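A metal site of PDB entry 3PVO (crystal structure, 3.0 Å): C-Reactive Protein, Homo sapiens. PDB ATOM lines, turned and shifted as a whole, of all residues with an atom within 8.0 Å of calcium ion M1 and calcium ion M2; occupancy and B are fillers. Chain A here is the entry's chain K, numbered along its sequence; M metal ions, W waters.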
ATOM      1  N   SER A  50     -15.752 -18.954   8.259  1.00  0.00           N
ATOM      2  CA  SER A  50     -14.524 -18.195   8.344  1.00  0.00           C
ATOM      3  C   SER A  50     -14.361 -17.588   9.729  1.00  0.00           C
ATOM      4  O   SER A  50     -15.286 -16.990  10.268  1.00  0.00           O
ATOM      5  CB  SER A  50     -14.509 -17.068   7.301  1.00  0.00           C
ATOM      6  OG  SER A  50     -13.383 -16.227   7.487  1.00  0.00           O
ATOM      7  N   SER A  53     -10.297 -13.621   8.091  1.00  0.00           N
ATOM      8  CA  SER A  53     -10.024 -13.519   6.660  1.00  0.00           C
ATOM      9  C   SER A  53      -9.124 -12.341   6.395  1.00  0.00           C
ATOM     10  O   SER A  53      -9.485 -11.192   6.675  1.00  0.00           O
ATOM     11  CB  SER A  53     -11.344 -13.362   5.907  1.00  0.00           C
ATOM     12  OG  SER A  53     -11.180 -13.180   4.509  1.00  0.00           O
ATOM     13  N   GLN A  59      -4.226 -11.835  -3.672  1.00  0.00           N
ATOM     14  CA  GLN A  59      -4.535 -13.124  -3.066  1.00  0.00           C
ATOM     15  C   GLN A  59      -5.674 -13.006  -2.062  1.00  0.00           C
ATOM     16  O   GLN A  59      -5.559 -12.315  -1.053  1.00  0.00           O
ATOM     17  CB  GLN A  59      -3.317 -13.704  -2.348  1.00  0.00           C
ATOM     18  CG  GLN A  59      -3.639 -14.905  -1.442  1.00  0.00           C
ATOM     19  CD  GLN A  59      -3.930 -16.158  -2.228  1.00  0.00           C
ATOM     20  OE1 GLN A  59      -5.047 -16.636  -2.246  1.00  0.00           O
ATOM     21  NE2 GLN A  59      -2.932 -16.671  -2.893  1.00  0.00           N
ATOM     22  N   ASP A  60      -6.766 -13.713  -2.349  1.00  0.00           N
ATOM     23  CA  ASP A  60      -7.956 -13.654  -1.497  1.00  0.00           C
ATOM     24  C   ASP A  60      -7.826 -14.423  -0.179  1.00  0.00           C
ATOM     25  O   ASP A  60      -8.511 -14.120   0.798  1.00  0.00           O
ATOM     26  CB  ASP A  60      -9.253 -13.966  -2.282  1.00  0.00           C
ATOM     27  CG  ASP A  60      -9.362 -15.422  -2.774  1.00  0.00           C
ATOM     28  OD1 ASP A  60      -8.528 -15.896  -3.600  1.00  0.00           O
ATOM     29  OD2 ASP A  60     -10.349 -16.080  -2.362  1.00  0.00           O
ATOM     30  N   ASN A  61      -6.932 -15.398  -0.123  1.00  0.00           N
ATOM     31  CA  ASN A  61      -6.703 -16.182   1.086  1.00  0.00           C
ATOM     32  C   ASN A  61      -5.276 -16.032   1.614  1.00  0.00           C
ATOM     33  O   ASN A  61      -4.607 -17.033   1.889  1.00  0.00           O
ATOM     34  CB  ASN A  61      -7.020 -17.660   0.818  1.00  0.00           C
ATOM     35  CG  ASN A  61      -8.487 -17.909   0.481  1.00  0.00           C
ATOM     36  OD1 ASN A  61      -9.314 -17.000   0.493  1.00  0.00           O
ATOM     37  ND2 ASN A  61      -8.815 -19.158   0.185  1.00  0.00           N
ATOM     38  N   LEU A  64      -5.895 -17.046   6.353  1.00  0.00           N
ATOM     39  CA  LEU A  64      -7.283 -17.448   6.591  1.00  0.00           C
ATOM     40  C   LEU A  64      -7.403 -18.542   7.619  1.00  0.00           C
ATOM     41  O   LEU A  64      -6.937 -19.677   7.388  1.00  0.00           O
ATOM     42  CB  LEU A  64      -7.970 -17.915   5.296  1.00  0.00           C
ATOM     43  CG  LEU A  64      -9.403 -18.479   5.431  1.00  0.00           C
ATOM     44  CD1 LEU A  64     -10.413 -17.360   5.706  1.00  0.00           C
ATOM     45  CD2 LEU A  64      -9.813 -19.273   4.190  1.00  0.00           C
ATOM     46  N   PHE A  66     -10.085 -20.898   9.205  1.00  0.00           N
ATOM     47  CA  PHE A  66     -11.376 -21.381   8.783  1.00  0.00           C
ATOM     48  C   PHE A  66     -11.728 -22.615   9.575  1.00  0.00           C
ATOM     49  O   PHE A  66     -10.834 -23.350  10.003  1.00  0.00           O
ATOM     50  CB  PHE A  66     -11.286 -21.786   7.315  1.00  0.00           C
ATOM     51  CG  PHE A  66     -12.617 -21.935   6.613  1.00  0.00           C
ATOM     52  CD1 PHE A  66     -13.190 -20.904   5.962  1.00  0.00           C
ATOM     53  CD2 PHE A  66     -13.271 -23.103   6.589  1.00  0.00           C
ATOM     54  CE1 PHE A  66     -14.422 -21.045   5.314  1.00  0.00           C
ATOM     55  CE2 PHE A  66     -14.511 -23.224   5.935  1.00  0.00           C
ATOM     56  CZ  PHE A  66     -15.063 -22.199   5.303  1.00  0.00           C
ATOM     57  N   GLN A 137     -17.018 -13.063   7.649  1.00  0.00           N
ATOM     58  CA  GLN A 137     -17.213 -13.595   6.309  1.00  0.00           C
ATOM     59  C   GLN A 137     -15.920 -14.149   5.772  1.00  0.00           C
ATOM     60  O   GLN A 137     -14.848 -13.815   6.298  1.00  0.00           O
ATOM     61  CB  GLN A 137     -17.724 -12.516   5.356  1.00  0.00           C
ATOM     62  CG  GLN A 137     -19.032 -11.843   5.734  1.00  0.00           C
ATOM     63  CD  GLN A 137     -20.224 -12.758   5.597  1.00  0.00           C
ATOM     64  OE1 GLN A 137     -21.253 -12.541   6.221  1.00  0.00           O
ATOM     65  NE2 GLN A 137     -20.090 -13.789   4.752  1.00  0.00           N
ATOM     66  N   GLU A 138     -16.017 -14.970   4.716  1.00  0.00           N
ATOM     67  CA  GLU A 138     -14.841 -15.407   3.928  1.00  0.00           C
ATOM     68  C   GLU A 138     -14.730 -14.556   2.673  1.00  0.00           C
ATOM     69  O   GLU A 138     -15.674 -14.468   1.882  1.00  0.00           O
ATOM     70  CB  GLU A 138     -14.923 -16.890   3.558  1.00  0.00           C
ATOM     71  CG  GLU A 138     -13.579 -17.563   3.225  1.00  0.00           C
ATOM     72  CD  GLU A 138     -13.172 -17.473   1.753  1.00  0.00           C
ATOM     73  OE1 GLU A 138     -13.940 -17.949   0.877  1.00  0.00           O
ATOM     74  OE2 GLU A 138     -12.063 -16.964   1.443  1.00  0.00           O
ATOM     75  N   GLN A 139     -13.571 -13.920   2.492  1.00  0.00           N
ATOM     76  CA  GLN A 139     -13.355 -13.062   1.337  1.00  0.00           C
ATOM     77  C   GLN A 139     -13.071 -13.909   0.104  1.00  0.00           C
ATOM     78  O   GLN A 139     -12.359 -14.910   0.177  1.00  0.00           O
ATOM     79  CB  GLN A 139     -12.238 -12.048   1.592  1.00  0.00           C
ATOM     80  CG  GLN A 139     -12.612 -10.918   2.542  1.00  0.00           C
ATOM     81  CD  GLN A 139     -11.424 -10.047   2.901  1.00  0.00           C
ATOM     82  OE1 GLN A 139     -10.647 -10.376   3.799  1.00  0.00           O
ATOM     83  NE2 GLN A 139     -11.287  -8.930   2.217  1.00  0.00           N
ATOM     84  N   ASP A 140     -13.649 -13.497  -1.022  1.00  0.00           N
ATOM     85  CA  ASP A 140     -13.231 -14.017  -2.324  1.00  0.00           C
ATOM     86  C   ASP A 140     -12.711 -12.920  -3.259  1.00  0.00           C
ATOM     87  O   ASP A 140     -12.222 -13.222  -4.343  1.00  0.00           O
ATOM     88  CB  ASP A 140     -14.327 -14.851  -2.979  1.00  0.00           C
ATOM     89  CG  ASP A 140     -14.521 -16.197  -2.291  1.00  0.00           C
ATOM     90  OD1 ASP A 140     -13.603 -16.704  -1.634  1.00  0.00           O
ATOM     91  OD2 ASP A 140     -15.596 -16.777  -2.413  1.00  0.00           O
ATOM     92  N   SER A 141     -12.800 -11.659  -2.824  1.00  0.00           N
ATOM     93  CA  SER A 141     -12.074 -10.568  -3.466  1.00  0.00           C
ATOM     94  C   SER A 141     -11.576  -9.582  -2.409  1.00  0.00           C
ATOM     95  O   SER A 141     -11.972  -9.675  -1.243  1.00  0.00           O
ATOM     96  CB  SER A 141     -12.939  -9.860  -4.498  1.00  0.00           C
ATOM     97  OG  SER A 141     -13.841  -8.996  -3.864  1.00  0.00           O
ATOM     98  N   GLY A 144     -14.546  -8.204  -0.212  1.00  0.00           N
ATOM     99  CA  GLY A 144     -15.853  -8.518  -0.737  1.00  0.00           C
ATOM    100  C   GLY A 144     -16.004  -9.942  -1.206  1.00  0.00           C
ATOM    101  O   GLY A 144     -15.221 -10.825  -0.830  1.00  0.00           O
ATOM    102  N   ASN A 145     -17.023 -10.162  -2.028  1.00  0.00           N
ATOM    103  CA  ASN A 145     -17.389 -11.494  -2.526  1.00  0.00           C
ATOM    104  C   ASN A 145     -17.580 -12.535  -1.430  1.00  0.00           C
ATOM    105  O   ASN A 145     -16.844 -13.507  -1.332  1.00  0.00           O
ATOM    106  CB  ASN A 145     -16.416 -11.962  -3.603  1.00  0.00           C
ATOM    107  CG  ASN A 145     -16.707 -11.345  -4.942  1.00  0.00           C
ATOM    108  OD1 ASN A 145     -16.382 -10.208  -5.209  1.00  0.00           O
ATOM    109  ND2 ASN A 145     -17.339 -12.092  -5.778  1.00  0.00           N
ATOM    110  N   PHE A 146     -18.571 -12.290  -0.587  1.00  0.00           N
ATOM    111  CA  PHE A 146     -18.833 -13.168   0.546  1.00  0.00           C
ATOM    112  C   PHE A 146     -19.821 -14.233   0.120  1.00  0.00           C
ATOM    113  O   PHE A 146     -20.600 -14.024  -0.799  1.00  0.00           O
ATOM    114  CB  PHE A 146     -19.384 -12.368   1.745  1.00  0.00           C
ATOM    115  CG  PHE A 146     -18.602 -11.126   2.073  1.00  0.00           C
ATOM    116  CD1 PHE A 146     -17.243 -11.182   2.341  1.00  0.00           C
ATOM    117  CD2 PHE A 146     -19.233  -9.883   2.120  1.00  0.00           C
ATOM    118  CE1 PHE A 146     -16.522 -10.033   2.644  1.00  0.00           C
ATOM    119  CE2 PHE A 146     -18.521  -8.744   2.419  1.00  0.00           C
ATOM    120  CZ  PHE A 146     -17.164  -8.818   2.685  1.00  0.00           C
ATOM    121  N   GLU A 147     -19.742 -15.392   0.773  1.00  0.00           N
ATOM    122  CA  GLU A 147     -20.760 -16.418   0.630  1.00  0.00           C
ATOM    123  C   GLU A 147     -21.328 -16.642   2.002  1.00  0.00           C
ATOM    124  O   GLU A 147     -20.592 -16.801   2.983  1.00  0.00           O
ATOM    125  CB  GLU A 147     -20.172 -17.741   0.123  1.00  0.00           C
ATOM    126  CG  GLU A 147     -19.411 -17.625  -1.170  1.00  0.00           C
ATOM    127  CD  GLU A 147     -18.377 -18.720  -1.349  1.00  0.00           C
ATOM    128  OE1 GLU A 147     -18.652 -19.830  -1.755  1.00  0.00           O
ATOM    129  OE2 GLU A 147     -17.223 -18.471  -1.090  1.00  0.00           O
ATOM    130  N   GLY A 148     -22.651 -16.645   2.066  1.00  0.00           N
ATOM    131  CA  GLY A 148     -23.379 -16.803   3.332  1.00  0.00           C
ATOM    132  C   GLY A 148     -23.153 -18.125   4.003  1.00  0.00           C
ATOM    133  O   GLY A 148     -23.271 -18.245   5.214  1.00  0.00           O
ATOM    134  N   SER A 149     -22.831 -19.142   3.215  1.00  0.00           N
ATOM    135  CA  SER A 149     -22.626 -20.477   3.747  1.00  0.00           C
ATOM    136  C   SER A 149     -21.274 -20.608   4.452  1.00  0.00           C
ATOM    137  O   SER A 149     -20.980 -21.661   5.024  1.00  0.00           O
ATOM    138  CB  SER A 149     -22.766 -21.509   2.635  1.00  0.00           C
ATOM    139  OG  SER A 149     -21.737 -21.373   1.684  1.00  0.00           O
ATOM    140  N   GLN A 150     -20.467 -19.548   4.429  1.00  0.00           N
ATOM    141  CA  GLN A 150     -19.153 -19.550   5.095  1.00  0.00           C
ATOM    142  C   GLN A 150     -19.125 -18.530   6.229  1.00  0.00           C
ATOM    143  O   GLN A 150     -18.079 -18.282   6.841  1.00  0.00           O
ATOM    144  CB  GLN A 150     -18.020 -19.289   4.081  1.00  0.00           C
ATOM    145  CG  GLN A 150     -17.862 -20.407   3.050  1.00  0.00           C
ATOM    146  CD  GLN A 150     -16.658 -20.246   2.130  1.00  0.00           C
ATOM    147  OE1 GLN A 150     -16.390 -19.162   1.593  1.00  0.00           O
ATOM    148  NE2 GLN A 150     -15.939 -21.320   1.933  1.00  0.00           N
ATOM    149  N   SER A 151     -20.283 -17.946   6.517  1.00  0.00           N
ATOM    150  CA  SER A 151     -20.406 -16.835   7.447  1.00  0.00           C
ATOM    151  C   SER A 151     -20.407 -17.288   8.899  1.00  0.00           C
ATOM    152  O   SER A 151     -20.939 -18.338   9.242  1.00  0.00           O
ATOM    153  CB  SER A 151     -21.644 -16.010   7.083  1.00  0.00           C
ATOM    154  OG  SER A 151     -22.728 -16.225   7.975  1.00  0.00           O
HETATM  155 CA    CA M   1     -11.666 -17.864  -1.066  1.00  0.00          CA
HETATM  156 CA    CA M   2     -16.290 -17.523   0.314  1.00  0.00          CA
HETATM  157  O   HOH W   1     -13.050 -20.869  -0.020  1.00  0.00           O
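O of Gln 139 touches calcium ion M1, at 3.3 Å. Along chain A the residues within 4 Å of calcium ion M1 span positions 60 to 140. The nearest printed residue that does not touch calcium ion M1 is Gln 150 (5.6 Å).
The side-chain carboxylate (OE2) of Glu 147 lies close to the side-chain carboxylate (OD2) of Asp 140 (2.7 Å). The backbone NH of Ser 50 is in hydrogen-bond range of the backbone carbonyl oxygen of Gln 150. The backbone carbonyl oxygen (O) of Asn 145 is in hydrogen-bond range of the backbone NH (N) of Asp 140 (3.2 Å). OD1 of Asn 61 sits close to OE2 of Glu 138 (2.9 Å). OD2 of Asp 60 lies close to OD1 of Asn 61. The backbone NH (N) of Asn 61 lies within hydrogen-bond range of the side-chain amide oxygen (OE1) of Gln 59. The side-chain amide oxygen (OE1) of Gln 139 is in hydrogen-bond range of the side-chain hydroxyl (OG) of Ser 53.
Calcium ion M1 is bound by the side-chain carboxylate (OD1) of Asp 140 (2.3 Å), the side-chain carboxylate (OD2) of Asp 60 (2.6 Å) and the side-chain carboxylate (OE2) of Glu 138 (2.7 Å). Slightly farther from calcium ion M1 lies OD1 of Asn 61 (3.0 Å). Slightly farther from calcium ion M1 lies the side-chain carboxylate (OE1) of Glu 138 (3.0 Å).
Of the 20 residues printed, 4 come within 4 Å of calcium ion M2.
Calcium ion M2 is bound by the side-chain carboxylate of Glu 147 (1.9 Å), the side-chain amide oxygen of Gln 150 (2.1 Å) and the side-chain carboxylate of Glu 138 (2.5 Å). Slightly farther from calcium ion M2 lies the side-chain carboxylate (OD2) of Asp 140 (2.9 Å).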
